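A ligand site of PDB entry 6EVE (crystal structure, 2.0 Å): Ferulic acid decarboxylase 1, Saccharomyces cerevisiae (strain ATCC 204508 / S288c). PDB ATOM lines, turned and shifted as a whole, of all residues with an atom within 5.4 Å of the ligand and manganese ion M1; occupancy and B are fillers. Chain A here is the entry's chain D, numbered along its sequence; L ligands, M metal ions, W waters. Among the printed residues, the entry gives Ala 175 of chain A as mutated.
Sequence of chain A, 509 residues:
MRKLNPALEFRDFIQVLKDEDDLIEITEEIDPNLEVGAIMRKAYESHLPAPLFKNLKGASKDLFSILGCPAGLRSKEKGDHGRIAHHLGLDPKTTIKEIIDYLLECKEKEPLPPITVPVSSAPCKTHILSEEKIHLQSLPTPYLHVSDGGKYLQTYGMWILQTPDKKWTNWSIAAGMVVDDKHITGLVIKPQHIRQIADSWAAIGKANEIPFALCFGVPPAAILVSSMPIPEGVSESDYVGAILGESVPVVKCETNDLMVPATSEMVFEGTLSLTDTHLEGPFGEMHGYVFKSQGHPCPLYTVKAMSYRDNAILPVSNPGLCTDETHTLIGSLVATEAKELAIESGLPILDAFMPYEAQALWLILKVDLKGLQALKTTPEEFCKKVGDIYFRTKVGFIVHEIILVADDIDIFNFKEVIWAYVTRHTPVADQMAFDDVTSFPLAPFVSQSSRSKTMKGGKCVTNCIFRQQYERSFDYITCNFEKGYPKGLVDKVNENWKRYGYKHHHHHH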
ATOM      1  N   GLN A 154       5.251  -1.511 -15.932  1.00  0.00           N
ATOM      2  CA  GLN A 154       6.145  -1.764 -14.802  1.00  0.00           C
ATOM      3  C   GLN A 154       7.561  -1.187 -15.129  1.00  0.00           C
ATOM      4  O   GLN A 154       8.317  -1.767 -15.914  1.00  0.00           O
ATOM      5  CB  GLN A 154       6.143  -3.255 -14.428  1.00  0.00           C
ATOM      6  CG  GLN A 154       7.293  -3.821 -13.577  1.00  0.00           C
ATOM      7  CD  GLN A 154       7.648  -3.068 -12.294  1.00  0.00           C
ATOM      8  OE1 GLN A 154       7.372  -1.876 -12.158  1.00  0.00           O
ATOM      9  NE2 GLN A 154       8.336  -3.769 -11.346  1.00  0.00           N
ATOM     10  N   THR A 155       7.843  -0.011 -14.566  1.00  0.00           N
ATOM     11  CA  THR A 155       9.184   0.598 -14.564  1.00  0.00           C
ATOM     12  C   THR A 155       9.632   1.153 -13.242  1.00  0.00           C
ATOM     13  O   THR A 155      10.806   1.449 -13.114  1.00  0.00           O
ATOM     14  CB  THR A 155       9.333   1.769 -15.571  1.00  0.00           C
ATOM     15  OG1 THR A 155       8.360   2.778 -15.322  1.00  0.00           O
ATOM     16  CG2 THR A 155       9.184   1.283 -16.969  1.00  0.00           C
ATOM     17  N   TYR A 156       8.714   1.319 -12.260  1.00  0.00           N
ATOM     18  CA  TYR A 156       9.106   1.685 -10.900  1.00  0.00           C
ATOM     19  C   TYR A 156       8.158   1.110  -9.822  1.00  0.00           C
ATOM     20  O   TYR A 156       7.840   1.789  -8.840  1.00  0.00           O
ATOM     21  CB  TYR A 156       9.184   3.209 -10.800  1.00  0.00           C
ATOM     22  CG  TYR A 156      10.072   3.793  -9.723  1.00  0.00           C
ATOM     23  CD1 TYR A 156      11.462   3.830  -9.897  1.00  0.00           C
ATOM     24  CD2 TYR A 156       9.546   4.417  -8.609  1.00  0.00           C
ATOM     25  CE1 TYR A 156      12.321   4.365  -8.912  1.00  0.00           C
ATOM     26  CE2 TYR A 156      10.372   4.969  -7.649  1.00  0.00           C
ATOM     27  CZ  TYR A 156      11.780   4.962  -7.803  1.00  0.00           C
ATOM     28  OH  TYR A 156      12.667   5.539  -6.869  1.00  0.00           O
ATOM     29  N   TRP A 168      11.620 -17.132   2.525  1.00  0.00           N
ATOM     30  CA  TRP A 168      12.258 -15.958   1.897  1.00  0.00           C
ATOM     31  C   TRP A 168      11.266 -15.234   1.005  1.00  0.00           C
ATOM     32  O   TRP A 168      10.748 -15.803   0.063  1.00  0.00           O
ATOM     33  CB  TRP A 168      13.515 -16.399   1.112  1.00  0.00           C
ATOM     34  CG  TRP A 168      14.226 -15.359   0.342  1.00  0.00           C
ATOM     35  CD1 TRP A 168      14.249 -13.999   0.585  1.00  0.00           C
ATOM     36  CD2 TRP A 168      15.106 -15.579  -0.798  1.00  0.00           C
ATOM     37  NE1 TRP A 168      15.049 -13.358  -0.361  1.00  0.00           N
ATOM     38  CE2 TRP A 168      15.605 -14.302  -1.198  1.00  0.00           C
ATOM     39  CE3 TRP A 168      15.526 -16.718  -1.501  1.00  0.00           C
ATOM     40  CZ2 TRP A 168      16.464 -14.141  -2.308  1.00  0.00           C
ATOM     41  CZ3 TRP A 168      16.416 -16.547  -2.606  1.00  0.00           C
ATOM     42  CH2 TRP A 168      16.868 -15.275  -2.987  1.00  0.00           C
ATOM     43  N   ASN A 170      11.141 -12.115  -1.613  1.00  0.00           N
ATOM     44  CA  ASN A 170      11.973 -11.133  -2.343  1.00  0.00           C
ATOM     45  C   ASN A 170      11.140  -9.986  -2.957  1.00  0.00           C
ATOM     46  O   ASN A 170      10.071 -10.213  -3.501  1.00  0.00           O
ATOM     47  CB  ASN A 170      12.809 -11.831  -3.450  1.00  0.00           C
ATOM     48  CG  ASN A 170      14.025 -11.007  -3.905  1.00  0.00           C
ATOM     49  OD1 ASN A 170      13.981 -10.418  -4.976  1.00  0.00           O
ATOM     50  ND2 ASN A 170      15.078 -11.007  -3.146  1.00  0.00           N
ATOM     51  N   TRP A 171      11.670  -8.753  -2.849  1.00  0.00           N
ATOM     52  CA  TRP A 171      11.093  -7.568  -3.477  1.00  0.00           C
ATOM     53  C   TRP A 171      12.160  -7.049  -4.445  1.00  0.00           C
ATOM     54  O   TRP A 171      13.325  -6.813  -4.010  1.00  0.00           O
ATOM     55  CB  TRP A 171      10.763  -6.459  -2.459  1.00  0.00           C
ATOM     56  CG  TRP A 171       9.623  -6.761  -1.389  1.00  0.00           C
ATOM     57  CD1 TRP A 171       8.755  -7.829  -1.371  1.00  0.00           C
ATOM     58  CD2 TRP A 171       9.268  -5.946  -0.254  1.00  0.00           C
ATOM     59  NE1 TRP A 171       7.862  -7.715  -0.303  1.00  0.00           N
ATOM     60  CE2 TRP A 171       8.172  -6.579   0.406  1.00  0.00           C
ATOM     61  CE3 TRP A 171       9.759  -4.734   0.277  1.00  0.00           C
ATOM     62  CZ2 TRP A 171       7.575  -6.049   1.554  1.00  0.00           C
ATOM     63  CZ3 TRP A 171       9.155  -4.210   1.421  1.00  0.00           C
ATOM     64  CH2 TRP A 171       8.083  -4.866   2.042  1.00  0.00           C
ATOM     65  N   SER A 172      11.772  -6.822  -5.695  1.00  0.00           N
ATOM     66  CA  SER A 172      12.744  -6.331  -6.717  1.00  0.00           C
ATOM     67  C   SER A 172      12.063  -5.641  -7.886  1.00  0.00           C
ATOM     68  O   SER A 172      10.850  -5.795  -8.092  1.00  0.00           O
ATOM     69  CB  SER A 172      13.622  -7.468  -7.228  1.00  0.00           C
ATOM     70  OG  SER A 172      12.902  -8.400  -8.021  1.00  0.00           O
ATOM     71  N   ILE A 173      12.827  -4.829  -8.624  1.00  0.00           N
ATOM     72  CA  ILE A 173      12.298  -4.141  -9.805  1.00  0.00           C
ATOM     73  C   ILE A 173      12.874  -4.816 -11.056  1.00  0.00           C
ATOM     74  O   ILE A 173      14.081  -5.131 -11.082  1.00  0.00           O
ATOM     75  CB  ILE A 173      12.694  -2.648  -9.810  1.00  0.00           C
ATOM     76  CG1 ILE A 173      12.235  -1.939  -8.540  1.00  0.00           C
ATOM     77  CG2 ILE A 173      12.071  -1.924 -10.985  1.00  0.00           C
ATOM     78  CD1 ILE A 173      12.884  -0.585  -8.405  1.00  0.00           C
ATOM     79  N   ALA A 174      12.021  -5.009 -12.058  1.00  0.00           N
ATOM     80  CA  ALA A 174      12.434  -5.458 -13.446  1.00  0.00           C
ATOM     81  C   ALA A 174      11.348  -4.986 -14.407  1.00  0.00           C
ATOM     82  O   ALA A 174      10.169  -5.062 -14.043  1.00  0.00           O
ATOM     83  CB  ALA A 174      12.579  -6.984 -13.525  1.00  0.00           C
ATOM     84  N   ALA A 175      11.713  -4.552 -15.620  1.00  0.00           N
ATOM     85  CA  ALA A 175      10.739  -4.036 -16.542  1.00  0.00           C
ATOM     86  C   ALA A 175       9.673  -5.063 -16.970  1.00  0.00           C
ATOM     87  O   ALA A 175       9.932  -6.280 -17.016  1.00  0.00           O
ATOM     88  CB  ALA A 175      11.368  -3.443 -17.777  1.00  0.00           C
ATOM     89  N   LEU A 187      11.657  -9.675 -18.406  1.00  0.00           N
ATOM     90  CA  LEU A 187      12.939 -10.348 -18.241  1.00  0.00           C
ATOM     91  C   LEU A 187      13.035 -10.925 -16.768  1.00  0.00           C
ATOM     92  O   LEU A 187      12.731 -10.239 -15.767  1.00  0.00           O
ATOM     93  CB  LEU A 187      14.085  -9.385 -18.637  1.00  0.00           C
ATOM     94  N   ILE A 189      15.993 -13.195 -15.367  1.00  0.00           N
ATOM     95  CA  ILE A 189      17.314 -13.739 -15.755  1.00  0.00           C
ATOM     96  C   ILE A 189      18.233 -13.990 -14.585  1.00  0.00           C
ATOM     97  O   ILE A 189      18.225 -13.232 -13.628  1.00  0.00           O
ATOM     98  CB  ILE A 189      18.073 -12.787 -16.741  1.00  0.00           C
ATOM     99  CG1 ILE A 189      18.216 -11.333 -16.190  1.00  0.00           C
ATOM    100  CG2 ILE A 189      17.337 -12.746 -18.077  1.00  0.00           C
ATOM    101  CD1 ILE A 189      19.421 -10.523 -16.722  1.00  0.00           C
ATOM    102  N   GLN A 192      19.643 -12.829 -11.005  1.00  0.00           N
ATOM    103  CA  GLN A 192      18.675 -12.031 -10.230  1.00  0.00           C
ATOM    104  C   GLN A 192      17.801 -12.941  -9.361  1.00  0.00           C
ATOM    105  O   GLN A 192      17.426 -14.037  -9.783  1.00  0.00           O
ATOM    106  CB  GLN A 192      17.778 -11.174 -11.161  1.00  0.00           C
ATOM    107  CG  GLN A 192      18.565 -10.180 -12.041  1.00  0.00           C
ATOM    108  CD  GLN A 192      19.230  -9.040 -11.266  1.00  0.00           C
ATOM    109  OE1 GLN A 192      20.169  -9.224 -10.445  1.00  0.00           O
ATOM    110  NE2 GLN A 192      18.713  -7.840 -11.475  1.00  0.00           N
ATOM    111  N   HIS A 193      17.473 -12.462  -8.166  1.00  0.00           N
ATOM    112  CA  HIS A 193      16.763 -13.289  -7.162  1.00  0.00           C
ATOM    113  C   HIS A 193      15.377 -13.780  -7.601  1.00  0.00           C
ATOM    114  O   HIS A 193      14.893 -14.817  -7.155  1.00  0.00           O
ATOM    115  CB  HIS A 193      16.711 -12.571  -5.829  1.00  0.00           C
ATOM    116  CG  HIS A 193      18.042 -12.492  -5.150  1.00  0.00           C
ATOM    117  ND1 HIS A 193      18.281 -11.686  -4.071  1.00  0.00           N
ATOM    118  CD2 HIS A 193      19.220 -13.124  -5.419  1.00  0.00           C
ATOM    119  CE1 HIS A 193      19.546 -11.803  -3.706  1.00  0.00           C
ATOM    120  NE2 HIS A 193      20.133 -12.675  -4.502  1.00  0.00           N
ATOM    121  N   ILE A 194      14.736 -13.025  -8.445  1.00  0.00           N
ATOM    122  CA  ILE A 194      13.491 -13.401  -9.022  1.00  0.00           C
ATOM    123  C   ILE A 194      13.619 -14.692  -9.879  1.00  0.00           C
ATOM    124  O   ILE A 194      12.749 -15.555  -9.833  1.00  0.00           O
ATOM    125  CB  ILE A 194      12.899 -12.170  -9.777  1.00  0.00           C
ATOM    126  CG1 ILE A 194      11.501 -12.426 -10.258  1.00  0.00           C
ATOM    127  CG2 ILE A 194      13.758 -11.802 -10.965  1.00  0.00           C
ATOM    128  CD1 ILE A 194      10.794 -11.155 -10.674  1.00  0.00           C
ATOM    129  N   SER A 226      14.233  -2.491  -3.126  1.00  0.00           N
ATOM    130  CA  SER A 226      13.870  -3.337  -4.227  1.00  0.00           C
ATOM    131  C   SER A 226      14.932  -3.249  -5.386  1.00  0.00           C
ATOM    132  O   SER A 226      15.108  -4.223  -6.109  1.00  0.00           O
ATOM    133  CB  SER A 226      12.454  -2.990  -4.734  1.00  0.00           C
ATOM    134  OG  SER A 226      11.419  -3.171  -3.731  1.00  0.00           O
ATOM    135  N   SER A 227      15.607  -2.103  -5.553  1.00  0.00           N
ATOM    136  CA  SER A 227      16.703  -1.956  -6.523  1.00  0.00           C
ATOM    137  C   SER A 227      18.109  -2.289  -6.025  1.00  0.00           C
ATOM    138  O   SER A 227      19.063  -2.097  -6.770  1.00  0.00           O
ATOM    139  CB  SER A 227      16.760  -0.546  -7.109  1.00  0.00           C
ATOM    140  OG  SER A 227      17.798  -0.465  -8.102  1.00  0.00           O
ATOM    141  N   MET A 228      18.241  -2.730  -4.785  1.00  0.00           N
ATOM    142  CA  MET A 228      19.559  -2.956  -4.148  1.00  0.00           C
ATOM    143  C   MET A 228      19.900  -4.459  -4.072  1.00  0.00           C
ATOM    144  O   MET A 228      19.057  -5.285  -3.644  1.00  0.00           O
ATOM    145  CB  MET A 228      19.499  -2.416  -2.748  1.00  0.00           C
ATOM    146  CG  MET A 228      20.738  -2.520  -1.898  1.00  0.00           C
ATOM    147  SD  MET A 228      20.503  -1.447  -0.405  1.00  0.00           S
ATOM    148  CE  MET A 228      22.087  -1.725   0.386  1.00  0.00           C
ATOM    149  N   PRO A 229      21.119  -4.825  -4.477  1.00  0.00           N
ATOM    150  CA  PRO A 229      21.531  -6.252  -4.395  1.00  0.00           C
ATOM    151  C   PRO A 229      21.995  -6.674  -2.974  1.00  0.00           C
ATOM    152  O   PRO A 229      23.168  -6.935  -2.745  1.00  0.00           O
ATOM    153  CB  PRO A 229      22.681  -6.338  -5.452  1.00  0.00           C
ATOM    154  CG  PRO A 229      23.269  -4.926  -5.463  1.00  0.00           C
ATOM    155  CD  PRO A 229      22.092  -4.014  -5.263  1.00  0.00           C
ATOM    156  N   ILE A 230      21.053  -6.804  -2.030  1.00  0.00           N
ATOM    157  CA  ILE A 230      21.345  -7.295  -0.691  1.00  0.00           C
ATOM    158  C   ILE A 230      21.483  -8.822  -0.786  1.00  0.00           C
ATOM    159  O   ILE A 230      21.162  -9.411  -1.841  1.00  0.00           O
ATOM    160  CB  ILE A 230      20.249  -6.858   0.353  1.00  0.00           C
ATOM    161  CG1 ILE A 230      18.890  -7.610   0.140  1.00  0.00           C
ATOM    162  CG2 ILE A 230      20.001  -5.350   0.250  1.00  0.00           C
ATOM    163  CD1 ILE A 230      17.854  -7.359   1.211  1.00  0.00           C
ATOM    164  N   PRO A 231      21.973  -9.473   0.278  1.00  0.00           N
ATOM    165  CA  PRO A 231      22.294 -10.908   0.160  1.00  0.00           C
ATOM    166  C   PRO A 231      21.109 -11.836  -0.111  1.00  0.00           C
ATOM    167  O   PRO A 231      19.948 -11.483   0.189  1.00  0.00           O
ATOM    168  CB  PRO A 231      22.861 -11.250   1.535  1.00  0.00           C
ATOM    169  CG  PRO A 231      23.311  -9.945   2.129  1.00  0.00           C
ATOM    170  CD  PRO A 231      22.378  -8.927   1.587  1.00  0.00           C
ATOM    171  N   VAL A 234      17.847 -12.969   2.344  1.00  0.00           N
ATOM    172  CA  VAL A 234      17.372 -11.895   3.242  1.00  0.00           C
ATOM    173  C   VAL A 234      16.107 -11.321   2.569  1.00  0.00           C
ATOM    174  O   VAL A 234      16.158 -10.987   1.333  1.00  0.00           O
ATOM    175  CB  VAL A 234      18.434 -10.807   3.487  1.00  0.00           C
ATOM    176  CG1 VAL A 234      17.962  -9.789   4.530  1.00  0.00           C
ATOM    177  CG2 VAL A 234      19.735 -11.467   3.937  1.00  0.00           C
ATOM    178  N   GLU A 236      13.854  -8.475   1.770  1.00  0.00           N
ATOM    179  CA  GLU A 236      14.078  -7.026   1.726  1.00  0.00           C
ATOM    180  C   GLU A 236      13.224  -6.239   2.755  1.00  0.00           C
ATOM    181  O   GLU A 236      13.700  -5.238   3.308  1.00  0.00           O
ATOM    182  CB  GLU A 236      13.728  -6.486   0.352  1.00  0.00           C
ATOM    183  CG  GLU A 236      14.815  -6.631  -0.732  1.00  0.00           C
ATOM    184  CD  GLU A 236      14.915  -8.013  -1.337  1.00  0.00           C
ATOM    185  OE1 GLU A 236      14.028  -8.876  -1.121  1.00  0.00           O
ATOM    186  OE2 GLU A 236      15.890  -8.215  -2.048  1.00  0.00           O
ATOM    187  N   PHE A 283      13.109  -2.376 -25.496  1.00  0.00           N
ATOM    188  CA  PHE A 283      12.850  -1.309 -24.556  1.00  0.00           C
ATOM    189  C   PHE A 283      14.113  -0.429 -24.490  1.00  0.00           C
ATOM    190  O   PHE A 283      15.235  -0.921 -24.474  1.00  0.00           O
ATOM    191  CB  PHE A 283      12.491  -1.887 -23.214  1.00  0.00           C
ATOM    192  CG  PHE A 283      12.038  -0.884 -22.216  1.00  0.00           C
ATOM    193  CD1 PHE A 283      11.030   0.006 -22.515  1.00  0.00           C
ATOM    194  CD2 PHE A 283      12.614  -0.844 -20.949  1.00  0.00           C
ATOM    195  CE1 PHE A 283      10.604   0.945 -21.607  1.00  0.00           C
ATOM    196  CE2 PHE A 283      12.189   0.092 -20.003  1.00  0.00           C
ATOM    197  CZ  PHE A 283      11.186   0.984 -20.348  1.00  0.00           C
ATOM    198  N   SER A 317       9.782   5.386 -14.342  1.00  0.00           N
ATOM    199  CA  SER A 317      11.157   5.685 -14.771  1.00  0.00           C
ATOM    200  C   SER A 317      11.265   5.485 -16.282  1.00  0.00           C
ATOM    201  O   SER A 317      10.720   4.483 -16.806  1.00  0.00           O
ATOM    202  CB  SER A 317      12.181   4.799 -14.066  1.00  0.00           C
ATOM    203  OG  SER A 317      13.475   4.926 -14.667  1.00  0.00           O
ATOM    204  N   PRO A 319      14.323   5.203 -18.878  1.00  0.00           N
ATOM    205  CA  PRO A 319      15.784   5.137 -18.964  1.00  0.00           C
ATOM    206  C   PRO A 319      16.376   5.628 -20.261  1.00  0.00           C
ATOM    207  O   PRO A 319      15.757   5.518 -21.288  1.00  0.00           O
ATOM    208  CB  PRO A 319      16.119   3.650 -18.811  1.00  0.00           C
ATOM    209  CG  PRO A 319      14.856   2.965 -18.473  1.00  0.00           C
ATOM    210  CD  PRO A 319      13.708   3.860 -18.790  1.00  0.00           C
ATOM    211  N   GLU A 325      16.987   7.120 -13.042  1.00  0.00           N
ATOM    212  CA  GLU A 325      16.987   6.168 -11.925  1.00  0.00           C
ATOM    213  C   GLU A 325      17.872   4.940 -12.198  1.00  0.00           C
ATOM    214  O   GLU A 325      18.342   4.264 -11.261  1.00  0.00           O
ATOM    215  CB  GLU A 325      15.562   5.623 -11.646  1.00  0.00           C
ATOM    216  CG  GLU A 325      14.472   6.573 -11.170  1.00  0.00           C
ATOM    217  CD  GLU A 325      14.015   7.601 -12.159  1.00  0.00           C
ATOM    218  OE1 GLU A 325      14.053   7.333 -13.400  1.00  0.00           O
ATOM    219  OE2 GLU A 325      13.638   8.729 -11.629  1.00  0.00           O
ATOM    220  N   THR A 326      18.114   4.638 -13.471  1.00  0.00           N
ATOM    221  CA  THR A 326      19.023   3.531 -13.789  1.00  0.00           C
ATOM    222  C   THR A 326      20.512   3.865 -13.386  1.00  0.00           C
ATOM    223  O   THR A 326      21.356   2.956 -13.293  1.00  0.00           O
ATOM    224  CB  THR A 326      18.884   3.018 -15.284  1.00  0.00           C
ATOM    225  OG1 THR A 326      19.244   4.032 -16.246  1.00  0.00           O
ATOM    226  CG2 THR A 326      17.474   2.592 -15.547  1.00  0.00           C
ATOM    227  N   LEU A 329      19.985   5.152  -8.834  1.00  0.00           N
ATOM    228  CA  LEU A 329      19.705   4.000  -7.961  1.00  0.00           C
ATOM    229  C   LEU A 329      20.522   2.757  -8.273  1.00  0.00           C
ATOM    230  O   LEU A 329      21.218   2.267  -7.363  1.00  0.00           O
ATOM    231  CB  LEU A 329      18.152   3.661  -7.888  1.00  0.00           C
ATOM    232  CG  LEU A 329      17.164   4.745  -7.435  1.00  0.00           C
ATOM    233  CD1 LEU A 329      15.721   4.215  -7.506  1.00  0.00           C
ATOM    234  CD2 LEU A 329      17.454   5.240  -6.021  1.00  0.00           C
ATOM    235  N   ILE A 330      20.477   2.221  -9.512  1.00  0.00           N
ATOM    236  CA  ILE A 330      21.173   0.947  -9.811  1.00  0.00           C
ATOM    237  C   ILE A 330      22.672   1.110  -9.523  1.00  0.00           C
ATOM    238  O   ILE A 330      23.227   0.290  -8.802  1.00  0.00           O
ATOM    239  CB  ILE A 330      20.960   0.429 -11.256  1.00  0.00           C
ATOM    240  CG1 ILE A 330      19.466   0.300 -11.560  1.00  0.00           C
ATOM    241  CG2 ILE A 330      21.590  -0.952 -11.442  1.00  0.00           C
ATOM    242  CD1 ILE A 330      19.173  -0.172 -12.956  1.00  0.00           C
ATOM    243  N   LYS A 394      27.605 -11.666  -7.792  1.00  0.00           N
ATOM    244  CA  LYS A 394      26.422 -10.951  -8.299  1.00  0.00           C
ATOM    245  C   LYS A 394      26.533  -9.441  -8.212  1.00  0.00           C
ATOM    246  O   LYS A 394      26.012  -8.699  -9.074  1.00  0.00           O
ATOM    247  CB  LYS A 394      25.208 -11.467  -7.520  1.00  0.00           C
ATOM    248  CG  LYS A 394      23.928 -10.710  -7.702  1.00  0.00           C
ATOM    249  CD  LYS A 394      22.734 -11.500  -7.106  1.00  0.00           C
ATOM    250  CE  LYS A 394      21.392 -10.836  -7.440  1.00  0.00           C
ATOM    251  NZ  LYS A 394      21.156  -9.582  -6.679  1.00  0.00           N
HETATM  252  C1  LIG L   1      16.190  -1.040 -11.458  1.00  0.00           C
HETATM  253  C2  LIG L   1      15.522   0.168 -11.536  1.00  0.00           C
HETATM  254  C3  LIG L   1      14.836   0.527 -12.714  1.00  0.00           C
HETATM  255  C4  LIG L   1      16.637  -4.202 -13.426  1.00  0.00           C
HETATM  256  C5  LIG L   1      14.846  -0.368 -13.809  1.00  0.00           C
HETATM  257  N1  LIG L   1      15.729  -6.325 -14.995  1.00  0.00           N
HETATM  258  C6  LIG L   1      16.541  -6.559 -13.944  1.00  0.00           C
HETATM  259  C7  LIG L   1      13.799   1.226 -15.524  1.00  0.00           C
HETATM  260  C8  LIG L   1      14.084  -0.214 -15.064  1.00  0.00           C
HETATM  261  C9  LIG L   1      15.382  -2.053 -16.092  1.00  0.00           C
HETATM  262  O1  LIG L   1      16.871  -7.830 -13.586  1.00  0.00           O
HETATM  263  N2  LIG L   1      16.973  -5.515 -13.187  1.00  0.00           N
HETATM  264  C10 LIG L   1      15.328  -5.038 -15.293  1.00  0.00           C
HETATM  265  O2  LIG L   1      14.534  -4.935 -16.270  1.00  0.00           O
HETATM  266  C11 LIG L   1      15.788  -3.901 -14.502  1.00  0.00           C
HETATM  267  N3  LIG L   1      15.546  -2.540 -14.763  1.00  0.00           N
HETATM  268  C12 LIG L   1      14.724  -0.840 -16.237  1.00  0.00           C
HETATM  269  C13 LIG L   1      12.732  -0.940 -14.894  1.00  0.00           C
HETATM  270  C14 LIG L   1      15.511  -1.613 -13.677  1.00  0.00           C
HETATM  271  C15 LIG L   1      14.131   1.867 -12.758  1.00  0.00           C
HETATM  272  C16 LIG L   1      15.605   0.986 -10.295  1.00  0.00           C
HETATM  273  C17 LIG L   1      16.194  -1.951 -12.506  1.00  0.00           C
HETATM  274  N4  LIG L   1      16.857  -3.230 -12.429  1.00  0.00           N
HETATM  275  C18 LIG L   1      17.679  -3.581 -11.252  1.00  0.00           C
HETATM  276  C19 LIG L   1      17.256  -4.506 -10.143  1.00  0.00           C
HETATM  277  O3  LIG L   1      16.171  -3.967  -9.401  1.00  0.00           O
HETATM  278  C20 LIG L   1      18.503  -4.712  -9.291  1.00  0.00           C
HETATM  279  O4  LIG L   1      19.477  -5.536  -9.961  1.00  0.00           O
HETATM  280  C21 LIG L   1      18.099  -5.413  -8.012  1.00  0.00           C
HETATM  281  O5  LIG L   1      19.236  -5.679  -7.206  1.00  0.00           O
HETATM  282  C22 LIG L   1      17.302  -6.713  -8.251  1.00  0.00           C
HETATM  283  O6  LIG L   1      17.021  -7.270  -6.936  1.00  0.00           O
HETATM  284  P1  LIG L   1      17.548  -8.653  -6.336  1.00  0.00           P
HETATM  285  O7  LIG L   1      16.432  -8.953  -5.288  1.00  0.00           O
HETATM  286  O8  LIG L   1      17.368  -9.643  -7.448  1.00  0.00           O
HETATM  287  O9  LIG L   1      18.893  -8.598  -5.667  1.00  0.00           O
HETATM  288 MN    MN M   1      16.958  -9.900  -3.169  1.00  0.00          MN
HETATM  289 MN    MN M   2      16.311  -6.178  -4.187  1.00  0.00          MN
HETATM  290  O   HOH W   1      15.222  -8.182 -11.292  1.00  0.00           O
HETATM  291  O   HOH W   2      18.930  -8.677  -3.060  1.00  0.00           O
HETATM  292  O   HOH W   3      21.472  -7.573  -8.686  1.00  0.00           O
HETATM  293  O   HOH W   4      15.235  -9.770  -8.839  1.00  0.00           O
HETATM  294  O   HOH W   5      15.325 -10.400 -14.460  1.00  0.00           O
HETATM  295  O   HOH W   6      22.110  -4.411  -9.489  1.00  0.00           O
HETATM  296  O   HOH W   7      17.393 -10.713  -1.350  1.00  0.00           O
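Of the 31 residues printed, 3 come within 4 Å of manganese ion M1. The nearest printed residue that does not touch manganese ion M1 is Trp 168 (4.4 Å).
Water W2 lies within hydrogen-bond range of O9 of the ligand (2.6 Å), O of Ile 230 (2.6 Å) and O of Met 228 (3.4 Å). Water W4 lies within hydrogen-bond range of O8 of the ligand, OG of Ser 172 and N of Ile 194. Water W1 lies within hydrogen-bond range of an oxygen (O1) of the ligand and the backbone carbonyl oxygen (O) of Ile 173. Water W3 lies within hydrogen-bond range of OE1 of Gln 192 (2.7 Å), NZ of Lys 394 (2.9 Å) and O4 of the ligand (3.1 Å). Water W5 lies within hydrogen-bond range of the backbone carbonyl oxygen (O) of Leu 187 (2.9 Å), the backbone NH (N) of Ile 189 (3.0 Å) and an oxygen (O1) of the ligand (3.1 Å).
The backbone carbonyl oxygen of Ser 226 lies within hydrogen-bond range of an oxygen (O3) of the ligand, at 3.5 Å. An oxygen (O9) of the ligand is in salt-bridge range of the side-chain amino group of Lys 394 (2.7 Å). O3 of the ligand is in hydrogen-bond range of O of Ile 173 (2.9 Å). An oxygen (O2) of the ligand lies within hydrogen-bond range of the backbone NH (N) of Ala 175, 2.9 Å away. An oxygen (O1) of the ligand is in hydrogen-bond range of the side-chain amide nitrogen (NE2) of Gln 192 (2.8 Å). The backbone NH of His 193 lies within hydrogen-bond range of an oxygen (O8) of the ligand (2.9 Å).
N of Pro 229 lies close to O5 of the ligand, at 3.4 Å. Merely in contact with the ligand: Thr 155 (3.4 Å), Ser 172 (3.4 Å), Ser 227 (3.4 Å), Met 228 (3.4 Å), Ile 330 (3.4 Å), Ala 174 (3.5 Å), Pro 319 (3.6 Å), Ser 317 (3.7 Å), Thr 326 (3.9 Å) and Trp 171 (3.98 Å). Hydrophobic or aromatic side chains within 4 Å of the ligand: Ile 173, Ala 174, Ala 175, His 193, Pro 229, Pro 319 and Ile 330. Within 4 Å of the ligand: Thr 155, Asn 170, Trp 171, Ser 172, Ile 173, Ala 174, Ala 175, Gln 192, His 193, Ser 226, Ser 227, Met 228, Pro 229, Glu 236, Ser 317, Pro 319, Thr 326, Ile 330 and Lys 394.
The side-chain carboxylate of Glu 325 is in hydrogen-bond range of the side-chain hydroxyl of Ser 317 (2.8 Å). The backbone NH (N) of Ile 173 sits at hydrogen-bond distance from the backbone carbonyl oxygen (O) of Ser 226, at 3.4 Å. The side-chain hydroxyl of Thr 155 sits at hydrogen-bond distance from the backbone NH of Ser 317 (3.1 Å). The side-chain carboxylate (OE1) of Glu 236 is in hydrogen-bond range of the backbone NH (N) of Trp 171 (2.9 Å). The backbone NH (N) of Ile 330 sits at hydrogen-bond distance from the backbone carbonyl oxygen (O) of Glu 325.
Water W7 is bound to manganese ion M1 (2.0 Å). The side-chain amide nitrogen (ND2) of Asn 170 binds manganese ion M1 (2.2 Å). Manganese ion M1 is bound by OE2 of Glu 236, at 2.3 Å. Water W2 binds manganese ion M1 (2.3 Å). An oxygen (O7) of the ligand binds manganese ion M1 (2.4 Å). Manganese ion M1 is bound by a ring nitrogen (ND1) of His 193 (2.4 Å). Manganese ion M1 has six donor atoms within binding distance.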
